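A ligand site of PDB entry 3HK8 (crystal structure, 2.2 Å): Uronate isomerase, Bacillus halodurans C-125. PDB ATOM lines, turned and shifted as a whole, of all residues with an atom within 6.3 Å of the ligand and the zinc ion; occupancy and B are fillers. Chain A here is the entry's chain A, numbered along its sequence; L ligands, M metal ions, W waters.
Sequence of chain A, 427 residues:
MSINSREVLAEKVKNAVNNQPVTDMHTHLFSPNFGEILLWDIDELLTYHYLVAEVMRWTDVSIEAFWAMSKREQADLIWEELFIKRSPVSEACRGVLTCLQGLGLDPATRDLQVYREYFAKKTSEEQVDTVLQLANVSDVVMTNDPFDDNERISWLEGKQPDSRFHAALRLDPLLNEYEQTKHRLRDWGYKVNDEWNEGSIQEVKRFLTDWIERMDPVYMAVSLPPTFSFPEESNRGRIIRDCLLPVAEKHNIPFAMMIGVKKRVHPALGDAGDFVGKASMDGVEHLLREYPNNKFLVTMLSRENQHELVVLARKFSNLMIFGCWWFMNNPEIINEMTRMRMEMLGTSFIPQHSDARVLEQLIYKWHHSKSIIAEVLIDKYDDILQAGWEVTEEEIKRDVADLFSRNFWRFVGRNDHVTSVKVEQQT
Water W1 lies within hydrogen-bond range of O of Asp 271 (2.5 Å), OD2 of Asp 274 (2.7 Å) and O5 of the ligand (2.7 Å). Water W3 lies within hydrogen-bond range of O2 of the ligand (2.7 Å), OG of Ser 223 (3.0 Å) and NZ of Lys 263 (3.0 Å). Water W2 lies within hydrogen-bond range of O of Asp 355 (2.6 Å), OH of Tyr 48 (2.7 Å) and O6 of the ligand (2.9 Å).
O of Asp 271 sits at hydrogen-bond distance from ND1 of His 49 (3.4 Å). The guanidinium group of Arg 170 is in salt-bridge range of the side-chain carboxylate of Asp 172, 3.0 Å away. The side-chain carboxylate of Asp 355 lies close to the indole nitrogen of Trp 325, at 3.3 Å. A ring nitrogen (NE2) of His 353 lies within hydrogen-bond range of the side-chain carboxylate (OD2) of Asp 355, 3.0 Å away. The side-chain carboxylate of Asp 172 sits at hydrogen-bond distance from the side-chain hydroxyl of Ser 223. NH1 of Arg 357 is in salt-bridge range of OD2 of Asp 271 (3.7 Å). NE2 of His 26 lies close to SD of Met 258, 3.7 Å away. ND1 of His 26 sits close to OG1 of Thr 143, 3.5 Å away.
OH of Tyr 50 is in hydrogen-bond range of O7 of the ligand (2.8 Å). The guanidinium group (NH1) of Arg 170 lies within salt-bridge range of an oxygen (O2) of the ligand (3.5 Å). The guanidinium group of Arg 357 lies within hydrogen-bond range of an oxygen (O6) of the ligand (2.7 Å). NE2 of His 49 sits at hydrogen-bond distance from O6 of the ligand, at 2.8 Å. The indole nitrogen (NE1) of Trp 325 sits close to an oxygen (O3) of the ligand.
The zinc ion is bound by OD1 of Asp 355 (2.0 Å). A ring nitrogen (NE2) of His 28 is bound to the zinc ion (2.0 Å). O3 of the ligand is bound to the zinc ion (2.1 Å). NE2 of His 26 binds the zinc ion, 2.2 Å away. The zinc ion is bound by O1 of the ligand (2.2 Å).
Ser 223 touches the ligand (CB to O2, 3.9 Å). Met 258 touches the ligand. CG of Trp 326 touches O7 of the ligand, at 3.2 Å. 11 residues have an atom within 4 Å of the ligand: His 26, His 28, His 49, Tyr 50, Arg 170, Ser 223, Met 258, Trp 325, Trp 326, Asp 355 and Arg 357. The nearest printed residue that does not touch the ligand is Asp 271 (4.4 Å).
Three residues have an atom within 4 Å of the zinc ion: His 26, His 28 and Asp 355. Along chain A the residues within 4 Å of the zinc ion span positions 26 to 355.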
ATOM      1  N   HIS A  26     -23.046  -5.235  14.721  1.00  0.00           N
ATOM      2  CA  HIS A  26     -22.170  -4.113  14.426  1.00  0.00           C
ATOM      3  C   HIS A  26     -21.838  -3.305  15.670  1.00  0.00           C
ATOM      4  O   HIS A  26     -22.702  -2.636  16.238  1.00  0.00           O
ATOM      5  CB  HIS A  26     -22.740  -3.159  13.373  1.00  0.00           C
ATOM      6  CG  HIS A  26     -21.874  -1.954  13.142  1.00  0.00           C
ATOM      7  ND1 HIS A  26     -20.544  -2.051  12.789  1.00  0.00           N
ATOM      8  CD2 HIS A  26     -22.133  -0.633  13.274  1.00  0.00           C
ATOM      9  CE1 HIS A  26     -20.019  -0.844  12.716  1.00  0.00           C
ATOM     10  NE2 HIS A  26     -20.963   0.033  13.002  1.00  0.00           N
ATOM     11  N   THR A  27     -20.578  -3.382  16.078  1.00  0.00           N
ATOM     12  CA  THR A  27     -20.085  -2.654  17.244  1.00  0.00           C
ATOM     13  C   THR A  27     -18.660  -2.203  16.964  1.00  0.00           C
ATOM     14  O   THR A  27     -18.087  -2.520  15.910  1.00  0.00           O
ATOM     15  CB  THR A  27     -20.027  -3.530  18.513  1.00  0.00           C
ATOM     16  OG1 THR A  27     -18.888  -4.401  18.426  1.00  0.00           O
ATOM     17  CG2 THR A  27     -21.301  -4.371  18.663  1.00  0.00           C
ATOM     18  N   HIS A  28     -18.099  -1.475  17.912  1.00  0.00           N
ATOM     19  CA  HIS A  28     -16.729  -0.994  17.832  1.00  0.00           C
ATOM     20  C   HIS A  28     -16.035  -1.503  19.086  1.00  0.00           C
ATOM     21  O   HIS A  28     -15.199  -0.816  19.694  1.00  0.00           O
ATOM     22  CB  HIS A  28     -16.717   0.540  17.759  1.00  0.00           C
ATOM     23  CG  HIS A  28     -17.326   1.072  16.506  1.00  0.00           C
ATOM     24  ND1 HIS A  28     -16.619   1.186  15.330  1.00  0.00           N
ATOM     25  CD2 HIS A  28     -18.591   1.448  16.222  1.00  0.00           C
ATOM     26  CE1 HIS A  28     -17.424   1.600  14.369  1.00  0.00           C
ATOM     27  NE2 HIS A  28     -18.633   1.767  14.886  1.00  0.00           N
ATOM     28  N   TYR A  48     -17.761   9.293  25.884  1.00  0.00           N
ATOM     29  CA  TYR A  48     -18.279   8.784  24.600  1.00  0.00           C
ATOM     30  C   TYR A  48     -18.438  10.043  23.739  1.00  0.00           C
ATOM     31  O   TYR A  48     -18.897  11.070  24.241  1.00  0.00           O
ATOM     32  CB  TYR A  48     -19.625   8.115  24.883  1.00  0.00           C
ATOM     33  CG  TYR A  48     -20.387   7.537  23.716  1.00  0.00           C
ATOM     34  CD1 TYR A  48     -19.744   6.860  22.680  1.00  0.00           C
ATOM     35  CD2 TYR A  48     -21.794   7.563  23.718  1.00  0.00           C
ATOM     36  CE1 TYR A  48     -20.480   6.210  21.677  1.00  0.00           C
ATOM     37  CE2 TYR A  48     -22.533   6.922  22.729  1.00  0.00           C
ATOM     38  CZ  TYR A  48     -21.871   6.243  21.704  1.00  0.00           C
ATOM     39  OH  TYR A  48     -22.613   5.588  20.745  1.00  0.00           O
ATOM     40  N   HIS A  49     -18.093  10.000  22.458  1.00  0.00           N
ATOM     41  CA  HIS A  49     -18.188  11.222  21.661  1.00  0.00           C
ATOM     42  C   HIS A  49     -19.580  11.829  21.560  1.00  0.00           C
ATOM     43  O   HIS A  49     -19.709  13.042  21.347  1.00  0.00           O
ATOM     44  CB  HIS A  49     -17.527  11.058  20.274  1.00  0.00           C
ATOM     45  CG  HIS A  49     -18.352  10.304  19.273  1.00  0.00           C
ATOM     46  ND1 HIS A  49     -19.372  10.887  18.552  1.00  0.00           N
ATOM     47  CD2 HIS A  49     -18.261   9.030  18.828  1.00  0.00           C
ATOM     48  CE1 HIS A  49     -19.872  10.005  17.708  1.00  0.00           C
ATOM     49  NE2 HIS A  49     -19.216   8.864  17.847  1.00  0.00           N
ATOM     50  N   TYR A  50     -20.619  11.032  21.752  1.00  0.00           N
ATOM     51  CA  TYR A  50     -21.982  11.561  21.713  1.00  0.00           C
ATOM     52  C   TYR A  50     -22.135  12.590  22.835  1.00  0.00           C
ATOM     53  O   TYR A  50     -22.848  13.577  22.675  1.00  0.00           O
ATOM     54  CB  TYR A  50     -23.033  10.450  21.926  1.00  0.00           C
ATOM     55  CG  TYR A  50     -23.276   9.529  20.745  1.00  0.00           C
ATOM     56  CD1 TYR A  50     -22.217   9.064  19.968  1.00  0.00           C
ATOM     57  CD2 TYR A  50     -24.561   9.052  20.469  1.00  0.00           C
ATOM     58  CE1 TYR A  50     -22.431   8.152  18.933  1.00  0.00           C
ATOM     59  CE2 TYR A  50     -24.788   8.132  19.435  1.00  0.00           C
ATOM     60  CZ  TYR A  50     -23.712   7.687  18.676  1.00  0.00           C
ATOM     61  OH  TYR A  50     -23.906   6.750  17.682  1.00  0.00           O
ATOM     62  N   THR A 143     -15.561  -4.289  14.441  1.00  0.00           N
ATOM     63  CA  THR A 143     -15.295  -3.491  13.248  1.00  0.00           C
ATOM     64  C   THR A 143     -13.756  -3.558  13.214  1.00  0.00           C
ATOM     65  O   THR A 143     -13.085  -2.960  14.058  1.00  0.00           O
ATOM     66  CB  THR A 143     -15.727  -2.014  13.393  1.00  0.00           C
ATOM     67  OG1 THR A 143     -17.157  -1.946  13.446  1.00  0.00           O
ATOM     68  CG2 THR A 143     -15.243  -1.201  12.196  1.00  0.00           C
ATOM     69  N   ARG A 170     -13.532  -3.922   7.800  1.00  0.00           N
ATOM     70  CA  ARG A 170     -13.884  -2.540   7.486  1.00  0.00           C
ATOM     71  C   ARG A 170     -12.926  -2.034   6.408  1.00  0.00           C
ATOM     72  O   ARG A 170     -11.703  -2.154   6.552  1.00  0.00           O
ATOM     73  CB  ARG A 170     -13.790  -1.668   8.741  1.00  0.00           C
ATOM     74  CG  ARG A 170     -14.128  -0.190   8.486  1.00  0.00           C
ATOM     75  CD  ARG A 170     -15.538  -0.006   7.923  1.00  0.00           C
ATOM     76  NE  ARG A 170     -16.542   0.010   8.974  1.00  0.00           N
ATOM     77  CZ  ARG A 170     -17.147   1.108   9.424  1.00  0.00           C
ATOM     78  NH1 ARG A 170     -16.886   2.306   8.918  1.00  0.00           N
ATOM     79  NH2 ARG A 170     -18.006   1.011  10.435  1.00  0.00           N
ATOM     80  N   ASP A 172     -13.125   1.387   4.735  1.00  0.00           N
ATOM     81  CA  ASP A 172     -13.186   2.822   4.440  1.00  0.00           C
ATOM     82  C   ASP A 172     -11.934   3.424   3.773  1.00  0.00           C
ATOM     83  O   ASP A 172     -12.042   4.092   2.741  1.00  0.00           O
ATOM     84  CB  ASP A 172     -13.523   3.609   5.713  1.00  0.00           C
ATOM     85  CG  ASP A 172     -14.934   3.338   6.219  1.00  0.00           C
ATOM     86  OD1 ASP A 172     -15.504   2.284   5.851  1.00  0.00           O
ATOM     87  OD2 ASP A 172     -15.476   4.161   6.978  1.00  0.00           O
ATOM     88  N   SER A 223     -18.425   2.778   5.309  1.00  0.00           N
ATOM     89  CA  SER A 223     -19.380   3.844   5.562  1.00  0.00           C
ATOM     90  C   SER A 223     -19.218   4.746   4.330  1.00  0.00           C
ATOM     91  O   SER A 223     -18.098   4.983   3.875  1.00  0.00           O
ATOM     92  CB  SER A 223     -19.070   4.604   6.860  1.00  0.00           C
ATOM     93  OG  SER A 223     -17.825   5.266   6.821  1.00  0.00           O
ATOM     94  N   MET A 258     -22.965   1.477   5.041  1.00  0.00           N
ATOM     95  CA  MET A 258     -23.541   2.387   6.022  1.00  0.00           C
ATOM     96  C   MET A 258     -23.493   3.750   5.320  1.00  0.00           C
ATOM     97  O   MET A 258     -22.455   4.425   5.304  1.00  0.00           O
ATOM     98  CB  MET A 258     -22.699   2.365   7.307  1.00  0.00           C
ATOM     99  CG  MET A 258     -22.468   0.932   7.849  1.00  0.00           C
ATOM    100  SD  MET A 258     -21.756   0.789   9.515  1.00  0.00           S
ATOM    101  CE  MET A 258     -23.263   0.766  10.456  1.00  0.00           C
ATOM    102  N   VAL A 261     -23.180   9.422   5.847  1.00  0.00           N
ATOM    103  CA  VAL A 261     -22.321  10.200   6.741  1.00  0.00           C
ATOM    104  C   VAL A 261     -21.414  11.209   6.024  1.00  0.00           C
ATOM    105  O   VAL A 261     -20.704  10.859   5.094  1.00  0.00           O
ATOM    106  CB  VAL A 261     -21.434   9.266   7.617  1.00  0.00           C
ATOM    107  CG1 VAL A 261     -20.525   8.418   6.734  1.00  0.00           C
ATOM    108  CG2 VAL A 261     -20.617  10.085   8.588  1.00  0.00           C
ATOM    109  N   LYS A 263     -18.372  13.256   6.638  1.00  0.00           N
ATOM    110  CA  LYS A 263     -17.233  13.332   7.538  1.00  0.00           C
ATOM    111  C   LYS A 263     -16.654  14.713   7.815  1.00  0.00           C
ATOM    112  O   LYS A 263     -16.592  15.580   6.943  1.00  0.00           O
ATOM    113  CB  LYS A 263     -16.089  12.436   7.022  1.00  0.00           C
ATOM    114  CG  LYS A 263     -16.495  11.005   6.650  1.00  0.00           C
ATOM    115  CD  LYS A 263     -16.948  10.197   7.857  1.00  0.00           C
ATOM    116  CE  LYS A 263     -15.792   9.860   8.785  1.00  0.00           C
ATOM    117  NZ  LYS A 263     -16.215   9.047   9.959  1.00  0.00           N
ATOM    118  N   ASP A 271     -14.144  12.621  16.584  1.00  0.00           N
ATOM    119  CA  ASP A 271     -15.195  11.658  16.269  1.00  0.00           C
ATOM    120  C   ASP A 271     -16.607  12.233  16.379  1.00  0.00           C
ATOM    121  O   ASP A 271     -17.544  11.684  15.810  1.00  0.00           O
ATOM    122  CB  ASP A 271     -15.074  10.423  17.177  1.00  0.00           C
ATOM    123  CG  ASP A 271     -13.885   9.555  16.825  1.00  0.00           C
ATOM    124  OD1 ASP A 271     -13.470   9.546  15.640  1.00  0.00           O
ATOM    125  OD2 ASP A 271     -13.363   8.866  17.725  1.00  0.00           O
ATOM    126  N   ASP A 274     -18.872  14.519  12.796  1.00  0.00           N
ATOM    127  CA  ASP A 274     -19.527  14.082  11.565  1.00  0.00           C
ATOM    128  C   ASP A 274     -20.996  14.510  11.482  1.00  0.00           C
ATOM    129  O   ASP A 274     -21.703  14.551  12.495  1.00  0.00           O
ATOM    130  CB  ASP A 274     -19.414  12.558  11.399  1.00  0.00           C
ATOM    131  CG  ASP A 274     -17.982  12.084  11.303  1.00  0.00           C
ATOM    132  OD1 ASP A 274     -17.127  12.883  10.845  1.00  0.00           O
ATOM    133  OD2 ASP A 274     -17.706  10.921  11.677  1.00  0.00           O
ATOM    134  N   TRP A 325     -29.200   3.402  12.960  1.00  0.00           N
ATOM    135  CA  TRP A 325     -27.854   3.908  13.062  1.00  0.00           C
ATOM    136  C   TRP A 325     -27.562   5.343  13.501  1.00  0.00           C
ATOM    137  O   TRP A 325     -28.106   6.313  12.944  1.00  0.00           O
ATOM    138  CB  TRP A 325     -27.176   3.650  11.711  1.00  0.00           C
ATOM    139  CG  TRP A 325     -25.730   4.013  11.611  1.00  0.00           C
ATOM    140  CD1 TRP A 325     -24.762   3.802  12.554  1.00  0.00           C
ATOM    141  CD2 TRP A 325     -25.059   4.561  10.467  1.00  0.00           C
ATOM    142  NE1 TRP A 325     -23.524   4.184  12.055  1.00  0.00           N
ATOM    143  CE2 TRP A 325     -23.675   4.646  10.779  1.00  0.00           C
ATOM    144  CE3 TRP A 325     -25.490   4.986   9.199  1.00  0.00           C
ATOM    145  CZ2 TRP A 325     -22.734   5.147   9.876  1.00  0.00           C
ATOM    146  CZ3 TRP A 325     -24.549   5.475   8.303  1.00  0.00           C
ATOM    147  CH2 TRP A 325     -23.185   5.547   8.648  1.00  0.00           C
ATOM    148  N   TRP A 326     -26.703   5.457  14.513  1.00  0.00           N
ATOM    149  CA  TRP A 326     -26.193   6.734  15.004  1.00  0.00           C
ATOM    150  C   TRP A 326     -27.255   7.783  15.345  1.00  0.00           C
ATOM    151  O   TRP A 326     -27.899   7.721  16.395  1.00  0.00           O
ATOM    152  CB  TRP A 326     -25.266   7.258  13.902  1.00  0.00           C
ATOM    153  CG  TRP A 326     -24.162   8.190  14.289  1.00  0.00           C
ATOM    154  CD1 TRP A 326     -24.086   9.015  15.377  1.00  0.00           C
ATOM    155  CD2 TRP A 326     -22.998   8.466  13.489  1.00  0.00           C
ATOM    156  NE1 TRP A 326     -22.955   9.799  15.300  1.00  0.00           N
ATOM    157  CE2 TRP A 326     -22.273   9.477  14.152  1.00  0.00           C
ATOM    158  CE3 TRP A 326     -22.518   7.958  12.278  1.00  0.00           C
ATOM    159  CZ2 TRP A 326     -21.072   9.999  13.645  1.00  0.00           C
ATOM    160  CZ3 TRP A 326     -21.312   8.483  11.763  1.00  0.00           C
ATOM    161  CH2 TRP A 326     -20.619   9.486  12.452  1.00  0.00           C
ATOM    162  N   PHE A 327     -27.434   8.760  14.462  1.00  0.00           N
ATOM    163  CA  PHE A 327     -28.418   9.823  14.683  1.00  0.00           C
ATOM    164  C   PHE A 327     -29.857   9.300  14.603  1.00  0.00           C
ATOM    165  O   PHE A 327     -30.792  10.019  14.959  1.00  0.00           O
ATOM    166  CB  PHE A 327     -28.207  10.957  13.672  1.00  0.00           C
ATOM    167  CG  PHE A 327     -26.817  11.536  13.693  1.00  0.00           C
ATOM    168  CD1 PHE A 327     -26.254  11.993  14.887  1.00  0.00           C
ATOM    169  CD2 PHE A 327     -26.050  11.590  12.532  1.00  0.00           C
ATOM    170  CE1 PHE A 327     -24.940  12.496  14.930  1.00  0.00           C
ATOM    171  CE2 PHE A 327     -24.739  12.092  12.561  1.00  0.00           C
ATOM    172  CZ  PHE A 327     -24.187  12.543  13.757  1.00  0.00           C
ATOM    173  N   HIS A 353     -28.736  -2.819  16.201  1.00  0.00           N
ATOM    174  CA  HIS A 353     -27.349  -3.152  16.479  1.00  0.00           C
ATOM    175  C   HIS A 353     -26.976  -2.038  17.469  1.00  0.00           C
ATOM    176  O   HIS A 353     -27.600  -0.987  17.465  1.00  0.00           O
ATOM    177  CB  HIS A 353     -26.463  -3.109  15.215  1.00  0.00           C
ATOM    178  CG  HIS A 353     -26.266  -1.738  14.647  1.00  0.00           C
ATOM    179  ND1 HIS A 353     -27.131  -1.176  13.718  1.00  0.00           N
ATOM    180  CD2 HIS A 353     -25.303  -0.808  14.869  1.00  0.00           C
ATOM    181  CE1 HIS A 353     -26.694   0.028  13.400  1.00  0.00           C
ATOM    182  NE2 HIS A 353     -25.589   0.277  14.084  1.00  0.00           N
ATOM    183  N   ASP A 355     -23.646  -0.583  18.012  1.00  0.00           N
ATOM    184  CA  ASP A 355     -22.618   0.344  17.552  1.00  0.00           C
ATOM    185  C   ASP A 355     -21.796   0.769  18.772  1.00  0.00           C
ATOM    186  O   ASP A 355     -21.199   1.841  18.779  1.00  0.00           O
ATOM    187  CB  ASP A 355     -23.260   1.572  16.907  1.00  0.00           C
ATOM    188  CG  ASP A 355     -22.603   1.926  15.580  1.00  0.00           C
ATOM    189  OD1 ASP A 355     -21.361   1.973  15.514  1.00  0.00           O
ATOM    190  OD2 ASP A 355     -23.350   2.156  14.609  1.00  0.00           O
ATOM    191  N   ARG A 357     -19.105   1.595  21.445  1.00  0.00           N
ATOM    192  CA  ARG A 357     -17.699   1.980  21.414  1.00  0.00           C
ATOM    193  C   ARG A 357     -17.081   1.675  22.771  1.00  0.00           C
ATOM    194  O   ARG A 357     -15.874   1.468  22.885  1.00  0.00           O
ATOM    195  CB  ARG A 357     -17.552   3.482  21.114  1.00  0.00           C
ATOM    196  CG  ARG A 357     -17.547   3.820  19.641  1.00  0.00           C
ATOM    197  CD  ARG A 357     -17.726   5.302  19.425  1.00  0.00           C
ATOM    198  NE  ARG A 357     -17.521   5.688  18.035  1.00  0.00           N
ATOM    199  CZ  ARG A 357     -16.326   5.857  17.464  1.00  0.00           C
ATOM    200  NH1 ARG A 357     -15.215   5.665  18.157  1.00  0.00           N
ATOM    201  NH2 ARG A 357     -16.258   6.233  16.195  1.00  0.00           N
HETATM  202  O1  LIG L   1     -19.430   2.670  11.902  1.00  0.00           O
HETATM  203  C1  LIG L   1     -19.429   3.916  11.747  1.00  0.00           C
HETATM  204  O2  LIG L   1     -18.880   4.526  10.798  1.00  0.00           O
HETATM  205  C2  LIG L   1     -20.171   4.791  12.784  1.00  0.00           C
HETATM  206  O3  LIG L   1     -21.043   3.957  13.554  1.00  0.00           O
HETATM  207  C3  LIG L   1     -19.131   5.507  13.682  1.00  0.00           C
HETATM  208  O4  LIG L   1     -18.419   4.582  14.512  1.00  0.00           O
HETATM  209  C4  LIG L   1     -19.732   6.608  14.646  1.00  0.00           C
HETATM  210  O5  LIG L   1     -18.728   7.531  15.041  1.00  0.00           O
HETATM  211  C5  LIG L   1     -20.374   6.036  15.937  1.00  0.00           C
HETATM  212  O6  LIG L   1     -19.959   6.325  17.059  1.00  0.00           O
HETATM  213  N1  LIG L   1     -21.415   5.196  15.787  1.00  0.00           N
HETATM  214  O7  LIG L   1     -22.646   5.629  15.397  1.00  0.00           O
HETATM  215 ZN    ZN M   1     -20.330   1.957  13.759  1.00  0.00          ZN
HETATM  216  O   HOH W   1     -17.590   9.854  14.154  1.00  0.00           O
HETATM  217  O   HOH W   2     -21.292   4.409  18.725  1.00  0.00           O
HETATM  218  O   HOH W   3     -18.044   6.732   9.389  1.00  0.00           O
